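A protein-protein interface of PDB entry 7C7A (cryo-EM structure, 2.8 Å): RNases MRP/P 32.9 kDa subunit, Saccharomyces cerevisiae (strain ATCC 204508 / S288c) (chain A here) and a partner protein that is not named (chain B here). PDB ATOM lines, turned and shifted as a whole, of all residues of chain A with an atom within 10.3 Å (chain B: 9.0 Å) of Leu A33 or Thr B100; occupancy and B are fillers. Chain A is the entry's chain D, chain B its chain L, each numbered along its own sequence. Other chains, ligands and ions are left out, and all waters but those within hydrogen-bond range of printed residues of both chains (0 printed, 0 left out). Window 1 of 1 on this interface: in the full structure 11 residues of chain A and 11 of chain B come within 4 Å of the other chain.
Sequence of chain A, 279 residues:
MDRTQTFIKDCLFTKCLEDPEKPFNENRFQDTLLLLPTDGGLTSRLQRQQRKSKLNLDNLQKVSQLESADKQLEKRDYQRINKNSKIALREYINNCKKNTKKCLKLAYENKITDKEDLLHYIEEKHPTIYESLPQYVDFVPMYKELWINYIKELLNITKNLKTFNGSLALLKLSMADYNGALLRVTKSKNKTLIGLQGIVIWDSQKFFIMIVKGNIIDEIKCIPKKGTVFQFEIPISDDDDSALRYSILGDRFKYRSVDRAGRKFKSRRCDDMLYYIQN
NE of Arg B24 lies within hydrogen-bond range of O of Leu A34 (3.0 Å). The guanidinium group (NH1) of Arg B24 sits at hydrogen-bond distance from the backbone carbonyl oxygen (O) of Leu A36 (2.7 Å). The side-chain hydroxyl (OG1) of Thr B100 sits at hydrogen-bond distance from the backbone NH (N) of Gln A30 (3.2 Å). The side-chain hydroxyl of Thr B100 lies within hydrogen-bond range of the backbone carbonyl oxygen of Arg A28, at 3.0 Å.
O of Leu B101 is in hydrogen-bond range of OG1 of Thr B104 (2.5 Å). The side-chain carboxylate (OE2) of Glu A26 is in salt-bridge range of the guanidinium group (NE) of Arg A28 (3.8 Å). O of Cys B103 lies within hydrogen-bond range of OG1 of Thr B107, at 3.0 Å. The side-chain sulfur (SG) of Cys B103 is in hydrogen-bond range of the backbone carbonyl oxygen (O) of Thr B100 (3.1 Å). The backbone NH (N) of Arg A28 lies within hydrogen-bond range of the backbone carbonyl oxygen (O) of Pro A23 (2.9 Å). The backbone carbonyl oxygen of Leu B21 lies close to the side-chain amide oxygen of Asn B25, 3.2 Å away.
Among the printed residues, merely in contact across the chains: Phe A13 with Ile B93 (3.5 Å), Phe A29 with Cys B103 (3.6 Å), Leu A33 with Thr B104 (3.7 Å), Leu A35 with Leu B21 (3.7 Å), Leu A33 with Thr B100 (3.7 Å), Phe A29 with Thr B100 (3.7 Å), Phe A13 with Val B99 (3.8 Å), Leu A17 with Ile B93 (3.8 Å), Leu A35 with Arg B24 (3.9 Å) and Leu A35 with Leu B20 (3.9 Å).
Printed residues of chain B within 4 Å of Leu A17: Ile B93 (3.8 Å). Leu A33 touches just these residues of chain B: Thr B100 (3.7 Å) and Thr B104 (3.7 Å). Of the printed residues of chain B, Leu A35 touches Leu B20, Leu B21 and Arg B24. Of the printed residues of chain A, Leu B20 touches Leu A35 (3.9 Å). Of the printed residues of chain A, Ile B93 touches Phe A13 (3.5 Å) and Leu A17 (3.8 Å). Phe B98 touches none of the printed residues of chain A. Val B99 touches one residue of chain A. Thr B100 touches just these residues of chain A: Arg A28, Phe A29, Gln A30 and Leu A33. No residue of chain A comes within 4 Å of Leu B101. Leu B105 touches none of the printed residues of chain A. The nearest residue of chain B that does not touch Leu A33 is Leu B101 (4.8 Å).
Of the 17 printed residues of chain A, 9 touch a printed residue of chain B. Printed residues of chain A that touch a printed residue of chain B: Phe A13, Leu A17, Arg A28, Phe A29, Gln A30, Leu A33, Leu A34, Leu A35 and Leu A36. Hydrophobic or aromatic side chains of chain A that line the printed part of chain B: Phe A13, Leu A17, Phe A29, Leu A33 and Leu A35. Printed residues of chain B that touch a printed residue of chain A: Leu B20, Leu B21, Arg B24, Ile B93, Val B99, Thr B100, Cys B103 and Thr B104. Hydrophobic or aromatic side chains of chain B that line the printed part of chain A: Ile B93 and Val B99. Among the printed residues, no Asp or Glu carboxylate lies within 4 Å of a Lys or Arg side-chain nitrogen of the other chain.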
ATOM      1  N   LYS A   9      -6.113   6.571  35.859  1.00  0.00           N
ATOM      2  CA  LYS A   9      -6.144   7.771  35.025  1.00  0.00           C
ATOM      3  C   LYS A   9      -7.549   8.352  34.938  1.00  0.00           C
ATOM      4  O   LYS A   9      -7.719   9.575  34.928  1.00  0.00           O
ATOM      5  CB  LYS A   9      -5.614   7.465  33.623  1.00  0.00           C
ATOM      6  CG  LYS A   9      -4.125   7.724  33.419  1.00  0.00           C
ATOM      7  CD  LYS A   9      -3.282   6.580  33.939  1.00  0.00           C
ATOM      8  CE  LYS A   9      -1.830   6.709  33.515  1.00  0.00           C
ATOM      9  NZ  LYS A   9      -1.014   5.578  34.038  1.00  0.00           N
ATOM     10  N   LEU A  12      -8.436  10.041  38.101  1.00  0.00           N
ATOM     11  CA  LEU A  12      -7.689  11.290  38.150  1.00  0.00           C
ATOM     12  C   LEU A  12      -8.278  12.367  37.249  1.00  0.00           C
ATOM     13  O   LEU A  12      -8.320  13.534  37.650  1.00  0.00           O
ATOM     14  CB  LEU A  12      -6.227  11.041  37.763  1.00  0.00           C
ATOM     15  CG  LEU A  12      -5.295  12.252  37.726  1.00  0.00           C
ATOM     16  CD1 LEU A  12      -4.980  12.729  39.133  1.00  0.00           C
ATOM     17  CD2 LEU A  12      -4.019  11.914  36.971  1.00  0.00           C
ATOM     18  N   PHE A  13      -8.735  12.002  36.049  1.00  0.00           N
ATOM     19  CA  PHE A  13      -9.360  12.945  35.131  1.00  0.00           C
ATOM     20  C   PHE A  13     -10.751  13.374  35.572  1.00  0.00           C
ATOM     21  O   PHE A  13     -11.185  14.472  35.205  1.00  0.00           O
ATOM     22  CB  PHE A  13      -9.456  12.344  33.722  1.00  0.00           C
ATOM     23  CG  PHE A  13      -8.185  12.444  32.925  1.00  0.00           C
ATOM     24  CD1 PHE A  13      -7.636  13.677  32.620  1.00  0.00           C
ATOM     25  CD2 PHE A  13      -7.552  11.303  32.459  1.00  0.00           C
ATOM     26  CE1 PHE A  13      -6.471  13.769  31.881  1.00  0.00           C
ATOM     27  CE2 PHE A  13      -6.387  11.389  31.721  1.00  0.00           C
ATOM     28  CZ  PHE A  13      -5.847  12.623  31.431  1.00  0.00           C
ATOM     29  N   LEU A  17     -11.276  17.185  34.783  1.00  0.00           N
ATOM     30  CA  LEU A  17     -12.279  17.293  33.736  1.00  0.00           C
ATOM     31  C   LEU A  17     -13.654  16.885  34.263  1.00  0.00           C
ATOM     32  O   LEU A  17     -13.791  16.259  35.317  1.00  0.00           O
ATOM     33  CB  LEU A  17     -11.895  16.430  32.535  1.00  0.00           C
ATOM     34  CG  LEU A  17     -10.698  16.898  31.705  1.00  0.00           C
ATOM     35  CD1 LEU A  17     -10.349  15.867  30.643  1.00  0.00           C
ATOM     36  CD2 LEU A  17     -10.979  18.251  31.072  1.00  0.00           C
ATOM     37  N   PRO A  23     -11.288  12.148  26.590  1.00  0.00           N
ATOM     38  CA  PRO A  23     -10.042  12.001  25.819  1.00  0.00           C
ATOM     39  C   PRO A  23      -9.803  10.586  25.324  1.00  0.00           C
ATOM     40  O   PRO A  23      -9.323  10.404  24.199  1.00  0.00           O
ATOM     41  CB  PRO A  23      -8.956  12.444  26.813  1.00  0.00           C
ATOM     42  CG  PRO A  23      -9.685  13.109  27.940  1.00  0.00           C
ATOM     43  CD  PRO A  23     -10.991  12.403  28.011  1.00  0.00           C
ATOM     44  N   PHE A  24     -10.118   9.576  26.138  1.00  0.00           N
ATOM     45  CA  PHE A  24      -9.931   8.196  25.704  1.00  0.00           C
ATOM     46  C   PHE A  24     -10.851   7.856  24.538  1.00  0.00           C
ATOM     47  O   PHE A  24     -10.526   6.998  23.709  1.00  0.00           O
ATOM     48  CB  PHE A  24     -10.165   7.240  26.874  1.00  0.00           C
ATOM     49  CG  PHE A  24      -9.058   7.244  27.890  1.00  0.00           C
ATOM     50  CD1 PHE A  24      -7.983   6.378  27.766  1.00  0.00           C
ATOM     51  CD2 PHE A  24      -9.091   8.112  28.968  1.00  0.00           C
ATOM     52  CE1 PHE A  24      -6.962   6.379  28.698  1.00  0.00           C
ATOM     53  CE2 PHE A  24      -8.073   8.118  29.904  1.00  0.00           C
ATOM     54  CZ  PHE A  24      -7.008   7.249  29.769  1.00  0.00           C
ATOM     55  N   GLU A  26     -11.978  10.289  22.244  1.00  0.00           N
ATOM     56  CA  GLU A  26     -11.493  11.062  21.107  1.00  0.00           C
ATOM     57  C   GLU A  26      -9.987  10.939  20.900  1.00  0.00           C
ATOM     58  O   GLU A  26      -9.428  11.683  20.088  1.00  0.00           O
ATOM     59  CB  GLU A  26     -11.880  12.538  21.257  1.00  0.00           C
ATOM     60  CG  GLU A  26     -11.182  13.265  22.389  1.00  0.00           C
ATOM     61  CD  GLU A  26     -11.610  14.715  22.497  1.00  0.00           C
ATOM     62  OE1 GLU A  26     -12.466  15.145  21.696  1.00  0.00           O
ATOM     63  OE2 GLU A  26     -11.088  15.426  23.382  1.00  0.00           O
ATOM     64  N   ASN A  27      -9.328  10.023  21.609  1.00  0.00           N
ATOM     65  CA  ASN A  27      -7.917   9.693  21.400  1.00  0.00           C
ATOM     66  C   ASN A  27      -7.019  10.923  21.559  1.00  0.00           C
ATOM     67  O   ASN A  27      -6.362  11.378  20.622  1.00  0.00           O
ATOM     68  CB  ASN A  27      -7.712   9.036  20.033  1.00  0.00           C
ATOM     69  CG  ASN A  27      -8.662   7.878  19.795  1.00  0.00           C
ATOM     70  OD1 ASN A  27      -8.462   6.780  20.313  1.00  0.00           O
ATOM     71  ND2 ASN A  27      -9.704   8.119  19.008  1.00  0.00           N
ATOM     72  N   ARG A  28      -7.002  11.458  22.779  1.00  0.00           N
ATOM     73  CA  ARG A  28      -6.131  12.571  23.125  1.00  0.00           C
ATOM     74  C   ARG A  28      -5.101  12.214  24.187  1.00  0.00           C
ATOM     75  O   ARG A  28      -4.256  13.052  24.518  1.00  0.00           O
ATOM     76  CB  ARG A  28      -6.960  13.772  23.597  1.00  0.00           C
ATOM     77  CG  ARG A  28      -7.850  14.363  22.519  1.00  0.00           C
ATOM     78  CD  ARG A  28      -7.416  15.766  22.133  1.00  0.00           C
ATOM     79  NE  ARG A  28      -8.264  16.321  21.082  1.00  0.00           N
ATOM     80  CZ  ARG A  28      -8.119  17.536  20.565  1.00  0.00           C
ATOM     81  NH1 ARG A  28      -8.939  17.955  19.611  1.00  0.00           N
ATOM     82  NH2 ARG A  28      -7.153  18.334  21.001  1.00  0.00           N
ATOM     83  N   PHE A  29      -5.143  10.996  24.727  1.00  0.00           N
ATOM     84  CA  PHE A  29      -4.173  10.554  25.727  1.00  0.00           C
ATOM     85  C   PHE A  29      -3.115   9.718  25.018  1.00  0.00           C
ATOM     86  O   PHE A  29      -3.261   8.508  24.838  1.00  0.00           O
ATOM     87  CB  PHE A  29      -4.861   9.773  26.840  1.00  0.00           C
ATOM     88  CG  PHE A  29      -3.924   9.293  27.913  1.00  0.00           C
ATOM     89  CD1 PHE A  29      -3.433  10.172  28.864  1.00  0.00           C
ATOM     90  CD2 PHE A  29      -3.538   7.964  27.972  1.00  0.00           C
ATOM     91  CE1 PHE A  29      -2.572   9.734  29.854  1.00  0.00           C
ATOM     92  CE2 PHE A  29      -2.677   7.520  28.959  1.00  0.00           C
ATOM     93  CZ  PHE A  29      -2.194   8.407  29.901  1.00  0.00           C
ATOM     94  N   GLN A  30      -2.034  10.377  24.605  1.00  0.00           N
ATOM     95  CA  GLN A  30      -0.959   9.699  23.893  1.00  0.00           C
ATOM     96  C   GLN A  30      -0.232   8.748  24.834  1.00  0.00           C
ATOM     97  O   GLN A  30       0.153   9.132  25.943  1.00  0.00           O
ATOM     98  CB  GLN A  30       0.014  10.719  23.307  1.00  0.00           C
ATOM     99  CG  GLN A  30      -0.652  11.872  22.577  1.00  0.00           C
ATOM    100  CD  GLN A  30       0.253  13.083  22.457  1.00  0.00           C
ATOM    101  OE1 GLN A  30       1.474  12.971  22.564  1.00  0.00           O
ATOM    102  NE2 GLN A  30      -0.343  14.248  22.236  1.00  0.00           N
ATOM    103  N   ASP A  31      -0.050   7.502  24.394  1.00  0.00           N
ATOM    104  CA  ASP A  31       0.671   6.520  25.196  1.00  0.00           C
ATOM    105  C   ASP A  31       2.182   6.684  25.113  1.00  0.00           C
ATOM    106  O   ASP A  31       2.900   6.103  25.933  1.00  0.00           O
ATOM    107  CB  ASP A  31       0.272   5.101  24.774  1.00  0.00           C
ATOM    108  CG  ASP A  31       0.581   4.808  23.316  1.00  0.00           C
ATOM    109  OD1 ASP A  31       1.046   5.718  22.600  1.00  0.00           O
ATOM    110  OD2 ASP A  31       0.357   3.658  22.884  1.00  0.00           O
ATOM    111  N   THR A  32       2.680   7.454  24.147  1.00  0.00           N
ATOM    112  CA  THR A  32       4.113   7.629  23.937  1.00  0.00           C
ATOM    113  C   THR A  32       4.452   9.111  23.953  1.00  0.00           C
ATOM    114  O   THR A  32       3.735   9.922  23.356  1.00  0.00           O
ATOM    115  CB  THR A  32       4.554   7.001  22.608  1.00  0.00           C
ATOM    116  OG1 THR A  32       4.301   5.591  22.635  1.00  0.00           O
ATOM    117  CG2 THR A  32       6.035   7.239  22.363  1.00  0.00           C
ATOM    118  N   LEU A  33       5.544   9.461  24.631  1.00  0.00           N
ATOM    119  CA  LEU A  33       6.074  10.819  24.646  1.00  0.00           C
ATOM    120  C   LEU A  33       7.416  10.829  23.928  1.00  0.00           C
ATOM    121  O   LEU A  33       8.400  10.280  24.436  1.00  0.00           O
ATOM    122  CB  LEU A  33       6.229  11.336  26.076  1.00  0.00           C
ATOM    123  CG  LEU A  33       4.953  11.734  26.817  1.00  0.00           C
ATOM    124  CD1 LEU A  33       5.261  12.038  28.272  1.00  0.00           C
ATOM    125  CD2 LEU A  33       4.296  12.930  26.146  1.00  0.00           C
ATOM    126  N   LEU A  34       7.457  11.460  22.757  1.00  0.00           N
ATOM    127  CA  LEU A  34       8.682  11.537  21.971  1.00  0.00           C
ATOM    128  C   LEU A  34       9.592  12.609  22.557  1.00  0.00           C
ATOM    129  O   LEU A  34       9.142  13.723  22.843  1.00  0.00           O
ATOM    130  CB  LEU A  34       8.359  11.837  20.509  1.00  0.00           C
ATOM    131  CG  LEU A  34       9.544  11.894  19.542  1.00  0.00           C
ATOM    132  CD1 LEU A  34      10.247  10.547  19.471  1.00  0.00           C
ATOM    133  CD2 LEU A  34       9.089  12.337  18.159  1.00  0.00           C
ATOM    134  N   LEU A  35      10.865  12.272  22.744  1.00  0.00           N
ATOM    135  CA  LEU A  35      11.866  13.190  23.285  1.00  0.00           C
ATOM    136  C   LEU A  35      13.061  13.192  22.334  1.00  0.00           C
ATOM    137  O   LEU A  35      13.919  12.307  22.396  1.00  0.00           O
ATOM    138  CB  LEU A  35      12.272  12.790  24.704  1.00  0.00           C
ATOM    139  CG  LEU A  35      11.191  12.948  25.775  1.00  0.00           C
ATOM    140  CD1 LEU A  35      11.598  12.250  27.064  1.00  0.00           C
ATOM    141  CD2 LEU A  35      10.891  14.418  26.025  1.00  0.00           C
ATOM    142  N   LEU A  36      13.116  14.198  21.458  1.00  0.00           N
ATOM    143  CA  LEU A  36      14.181  14.302  20.471  1.00  0.00           C
ATOM    144  C   LEU A  36      14.294  15.746  20.022  1.00  0.00           C
ATOM    145  O   LEU A  36      13.258  16.405  19.848  1.00  0.00           O
ATOM    146  CB  LEU A  36      13.907  13.401  19.261  1.00  0.00           C
ATOM    147  CG  LEU A  36      14.986  13.368  18.174  1.00  0.00           C
ATOM    148  CD1 LEU A  36      16.211  12.592  18.640  1.00  0.00           C
ATOM    149  CD2 LEU A  36      14.439  12.804  16.871  1.00  0.00           C
ATOM    150  N   LEU B  17      14.983  13.186  33.588  1.00  0.00           N
ATOM    151  CA  LEU B  17      13.753  13.239  32.804  1.00  0.00           C
ATOM    152  C   LEU B  17      13.184  14.651  32.765  1.00  0.00           C
ATOM    153  O   LEU B  17      12.676  15.095  31.724  1.00  0.00           O
ATOM    154  CB  LEU B  17      12.723  12.263  33.370  1.00  0.00           C
ATOM    155  CG  LEU B  17      12.846  10.805  32.930  1.00  0.00           C
ATOM    156  CD1 LEU B  17      12.175   9.885  33.937  1.00  0.00           C
ATOM    157  CD2 LEU B  17      12.256  10.612  31.542  1.00  0.00           C
ATOM    158  N   LEU B  20      15.244  16.511  30.276  1.00  0.00           N
ATOM    159  CA  LEU B  20      15.032  16.003  28.926  1.00  0.00           C
ATOM    160  C   LEU B  20      13.715  16.495  28.341  1.00  0.00           C
ATOM    161  O   LEU B  20      13.657  16.857  27.161  1.00  0.00           O
ATOM    162  CB  LEU B  20      15.074  14.475  28.926  1.00  0.00           C
ATOM    163  CG  LEU B  20      16.461  13.830  28.880  1.00  0.00           C
ATOM    164  CD1 LEU B  20      16.345  12.315  28.810  1.00  0.00           C
ATOM    165  CD2 LEU B  20      17.263  14.365  27.703  1.00  0.00           C
ATOM    166  N   LEU B  21      12.648  16.521  29.143  1.00  0.00           N
ATOM    167  CA  LEU B  21      11.380  17.008  28.614  1.00  0.00           C
ATOM    168  C   LEU B  21      11.351  18.533  28.548  1.00  0.00           C
ATOM    169  O   LEU B  21      10.669  19.100  27.685  1.00  0.00           O
ATOM    170  CB  LEU B  21      10.211  16.459  29.437  1.00  0.00           C
ATOM    171  CG  LEU B  21      10.000  16.834  30.904  1.00  0.00           C
ATOM    172  CD1 LEU B  21       9.120  18.065  31.016  1.00  0.00           C
ATOM    173  CD2 LEU B  21       9.395  15.670  31.672  1.00  0.00           C
ATOM    174  N   ARG B  24      12.785  19.892  25.259  1.00  0.00           N
ATOM    175  CA  ARG B  24      11.874  19.791  24.127  1.00  0.00           C
ATOM    176  C   ARG B  24      10.657  20.698  24.254  1.00  0.00           C
ATOM    177  O   ARG B  24      10.148  21.181  23.238  1.00  0.00           O
ATOM    178  CB  ARG B  24      11.411  18.341  23.953  1.00  0.00           C
ATOM    179  CG  ARG B  24      10.664  18.075  22.658  1.00  0.00           C
ATOM    180  CD  ARG B  24      10.261  16.617  22.559  1.00  0.00           C
ATOM    181  NE  ARG B  24       9.177  16.401  21.606  1.00  0.00           N
ATOM    182  CZ  ARG B  24       9.340  16.333  20.288  1.00  0.00           C
ATOM    183  NH1 ARG B  24      10.548  16.463  19.758  1.00  0.00           N
ATOM    184  NH2 ARG B  24       8.292  16.133  19.500  1.00  0.00           N
ATOM    185  N   ASN B  25      10.179  20.950  25.471  1.00  0.00           N
ATOM    186  CA  ASN B  25       8.997  21.779  25.690  1.00  0.00           C
ATOM    187  C   ASN B  25       9.364  23.241  25.940  1.00  0.00           C
ATOM    188  O   ASN B  25       8.509  24.061  26.277  1.00  0.00           O
ATOM    189  CB  ASN B  25       8.163  21.234  26.845  1.00  0.00           C
ATOM    190  CG  ASN B  25       7.416  19.968  26.477  1.00  0.00           C
ATOM    191  OD1 ASN B  25       7.561  18.935  27.130  1.00  0.00           O
ATOM    192  ND2 ASN B  25       6.609  20.042  25.425  1.00  0.00           N
ATOM    193  N   VAL B  92      -3.639  22.809  34.214  1.00  0.00           N
ATOM    194  CA  VAL B  92      -3.187  22.542  32.853  1.00  0.00           C
ATOM    195  C   VAL B  92      -3.855  21.297  32.280  1.00  0.00           C
ATOM    196  O   VAL B  92      -3.913  21.139  31.053  1.00  0.00           O
ATOM    197  CB  VAL B  92      -1.654  22.410  32.795  1.00  0.00           C
ATOM    198  CG1 VAL B  92      -1.204  21.053  33.315  1.00  0.00           C
ATOM    199  CG2 VAL B  92      -1.147  22.644  31.379  1.00  0.00           C
ATOM    200  N   ILE B  93      -4.372  20.413  33.136  1.00  0.00           N
ATOM    201  CA  ILE B  93      -5.126  19.257  32.666  1.00  0.00           C
ATOM    202  C   ILE B  93      -6.604  19.599  32.520  1.00  0.00           C
ATOM    203  O   ILE B  93      -7.267  19.129  31.587  1.00  0.00           O
ATOM    204  CB  ILE B  93      -4.916  18.069  33.621  1.00  0.00           C
ATOM    205  CG1 ILE B  93      -3.453  17.623  33.610  1.00  0.00           C
ATOM    206  CG2 ILE B  93      -5.829  16.911  33.257  1.00  0.00           C
ATOM    207  CD1 ILE B  93      -3.115  16.636  34.706  1.00  0.00           C
ATOM    208  N   GLY B  96      -7.872  20.705  28.935  1.00  0.00           N
ATOM    209  CA  GLY B  96      -8.169  19.657  27.979  1.00  0.00           C
ATOM    210  C   GLY B  96      -7.325  19.688  26.725  1.00  0.00           C
ATOM    211  O   GLY B  96      -7.330  18.706  25.972  1.00  0.00           O
ATOM    212  N   GLN B  97      -6.602  20.780  26.471  1.00  0.00           N
ATOM    213  CA  GLN B  97      -5.774  20.862  25.272  1.00  0.00           C
ATOM    214  C   GLN B  97      -4.549  19.963  25.389  1.00  0.00           C
ATOM    215  O   GLN B  97      -4.277  19.139  24.509  1.00  0.00           O
ATOM    216  CB  GLN B  97      -5.361  22.314  25.021  1.00  0.00           C
ATOM    217  CG  GLN B  97      -6.366  23.116  24.211  1.00  0.00           C
ATOM    218  CD  GLN B  97      -6.091  24.606  24.254  1.00  0.00           C
ATOM    219  OE1 GLN B  97      -6.897  25.411  23.786  1.00  0.00           O
ATOM    220  NE2 GLN B  97      -4.949  24.982  24.816  1.00  0.00           N
ATOM    221  N   PHE B  98      -3.796  20.110  26.477  1.00  0.00           N
ATOM    222  CA  PHE B  98      -2.555  19.368  26.701  1.00  0.00           C
ATOM    223  C   PHE B  98      -2.648  18.662  28.050  1.00  0.00           C
ATOM    224  O   PHE B  98      -2.309  19.228  29.092  1.00  0.00           O
ATOM    225  CB  PHE B  98      -1.346  20.310  26.631  1.00  0.00           C
ATOM    226  CG  PHE B  98      -1.289  21.133  25.375  1.00  0.00           C
ATOM    227  CD1 PHE B  98      -1.780  22.428  25.357  1.00  0.00           C
ATOM    228  CD2 PHE B  98      -0.746  20.611  24.214  1.00  0.00           C
ATOM    229  CE1 PHE B  98      -1.729  23.187  24.203  1.00  0.00           C
ATOM    230  CE2 PHE B  98      -0.693  21.365  23.056  1.00  0.00           C
ATOM    231  CZ  PHE B  98      -1.185  22.655  23.052  1.00  0.00           C
ATOM    232  N   VAL B  99      -3.113  17.412  28.025  1.00  0.00           N
ATOM    233  CA  VAL B  99      -3.219  16.634  29.255  1.00  0.00           C
ATOM    234  C   VAL B  99      -2.183  15.516  29.289  1.00  0.00           C
ATOM    235  O   VAL B  99      -1.829  15.025  30.371  1.00  0.00           O
ATOM    236  CB  VAL B  99      -4.644  16.078  29.412  1.00  0.00           C
ATOM    237  CG1 VAL B  99      -5.640  17.213  29.565  1.00  0.00           C
ATOM    238  CG2 VAL B  99      -5.007  15.200  28.225  1.00  0.00           C
ATOM    239  N   THR B 100      -1.683  15.103  28.120  1.00  0.00           N
ATOM    240  CA  THR B 100      -0.749  13.982  28.053  1.00  0.00           C
ATOM    241  C   THR B 100       0.522  14.270  28.842  1.00  0.00           C
ATOM    242  O   THR B 100       1.004  13.411  29.589  1.00  0.00           O
ATOM    243  CB  THR B 100      -0.416  13.663  26.595  1.00  0.00           C
ATOM    244  OG1 THR B 100      -1.606  13.248  25.912  1.00  0.00           O
ATOM    245  CG2 THR B 100       0.617  12.549  26.514  1.00  0.00           C
ATOM    246  N   LEU B 101       1.081  15.471  28.691  1.00  0.00           N
ATOM    247  CA  LEU B 101       2.237  15.840  29.497  1.00  0.00           C
ATOM    248  C   LEU B 101       1.826  16.387  30.857  1.00  0.00           C
ATOM    249  O   LEU B 101       2.634  16.381  31.791  1.00  0.00           O
ATOM    250  CB  LEU B 101       3.108  16.861  28.759  1.00  0.00           C
ATOM    251  CG  LEU B 101       2.624  18.309  28.646  1.00  0.00           C
ATOM    252  CD1 LEU B 101       3.789  19.223  28.308  1.00  0.00           C
ATOM    253  CD2 LEU B 101       1.538  18.438  27.594  1.00  0.00           C
ATOM    254  N   GLY B 102       0.579  16.841  30.997  1.00  0.00           N
ATOM    255  CA  GLY B 102       0.126  17.340  32.285  1.00  0.00           C
ATOM    256  C   GLY B 102       0.051  16.255  33.341  1.00  0.00           C
ATOM    257  O   GLY B 102       0.460  16.463  34.489  1.00  0.00           O
ATOM    258  N   CYS B 103      -0.475  15.083  32.975  1.00  0.00           N
ATOM    259  CA  CYS B 103      -0.528  13.976  33.925  1.00  0.00           C
ATOM    260  C   CYS B 103       0.876  13.516  34.300  1.00  0.00           C
ATOM    261  O   CYS B 103       1.148  13.180  35.461  1.00  0.00           O
ATOM    262  CB  CYS B 103      -1.344  12.820  33.346  1.00  0.00           C
ATOM    263  SG  CYS B 103      -0.613  12.030  31.895  1.00  0.00           S
ATOM    264  N   THR B 104       1.791  13.508  33.328  1.00  0.00           N
ATOM    265  CA  THR B 104       3.175  13.145  33.613  1.00  0.00           C
ATOM    266  C   THR B 104       3.827  14.159  34.546  1.00  0.00           C
ATOM    267  O   THR B 104       4.624  13.798  35.413  1.00  0.00           O
ATOM    268  CB  THR B 104       3.973  13.028  32.314  1.00  0.00           C
ATOM    269  OG1 THR B 104       4.089  14.319  31.703  1.00  0.00           O
ATOM    270  CG2 THR B 104       3.285  12.077  31.357  1.00  0.00           C
ATOM    271  N   LEU B 105       3.491  15.439  34.382  1.00  0.00           N
ATOM    272  CA  LEU B 105       4.030  16.471  35.263  1.00  0.00           C
ATOM    273  C   LEU B 105       3.485  16.318  36.680  1.00  0.00           C
ATOM    274  O   LEU B 105       4.213  16.493  37.668  1.00  0.00           O
ATOM    275  CB  LEU B 105       3.702  17.851  34.691  1.00  0.00           C
ATOM    276  CG  LEU B 105       4.267  19.090  35.381  1.00  0.00           C
ATOM    277  CD1 LEU B 105       5.784  19.042  35.415  1.00  0.00           C
ATOM    278  CD2 LEU B 105       3.789  20.339  34.658  1.00  0.00           C
ATOM    279  N   VAL B 106       2.196  15.985  36.795  1.00  0.00           N
ATOM    280  CA  VAL B 106       1.600  15.726  38.106  1.00  0.00           C
ATOM    281  C   VAL B 106       2.297  14.548  38.777  1.00  0.00           C
ATOM    282  O   VAL B 106       2.614  14.580  39.973  1.00  0.00           O
ATOM    283  CB  VAL B 106       0.086  15.479  37.971  1.00  0.00           C
ATOM    284  CG1 VAL B 106      -0.487  14.944  39.275  1.00  0.00           C
ATOM    285  CG2 VAL B 106      -0.626  16.758  37.557  1.00  0.00           C
ATOM    286  N   THR B 107       2.557  13.490  38.005  1.00  0.00           N
ATOM    287  CA  THR B 107       3.241  12.320  38.549  1.00  0.00           C
ATOM    288  C   THR B 107       4.679  12.655  38.938  1.00  0.00           C
ATOM    289  O   THR B 107       5.200  12.154  39.943  1.00  0.00           O
ATOM    290  CB  THR B 107       3.203  11.175  37.534  1.00  0.00           C
ATOM    291  OG1 THR B 107       1.841  10.867  37.214  1.00  0.00           O
ATOM    292  CG2 THR B 107       3.872   9.932  38.101  1.00  0.00           C
ATOM    293  N   LEU B 108       5.335  13.508  38.148  1.00  0.00           N
ATOM    294  CA  LEU B 108       6.675  13.980  38.479  1.00  0.00           C
ATOM    295  C   LEU B 108       6.683  14.690  39.825  1.00  0.00           C
ATOM    296  O   LEU B 108       7.545  14.437  40.672  1.00  0.00           O
ATOM    297  CB  LEU B 108       7.188  14.914  37.380  1.00  0.00           C
ATOM    298  CG  LEU B 108       7.750  14.298  36.099  1.00  0.00           C
ATOM    299  CD1 LEU B 108       7.912  15.365  35.032  1.00  0.00           C
ATOM    300  CD2 LEU B 108       9.084  13.629  36.382  1.00  0.00           C
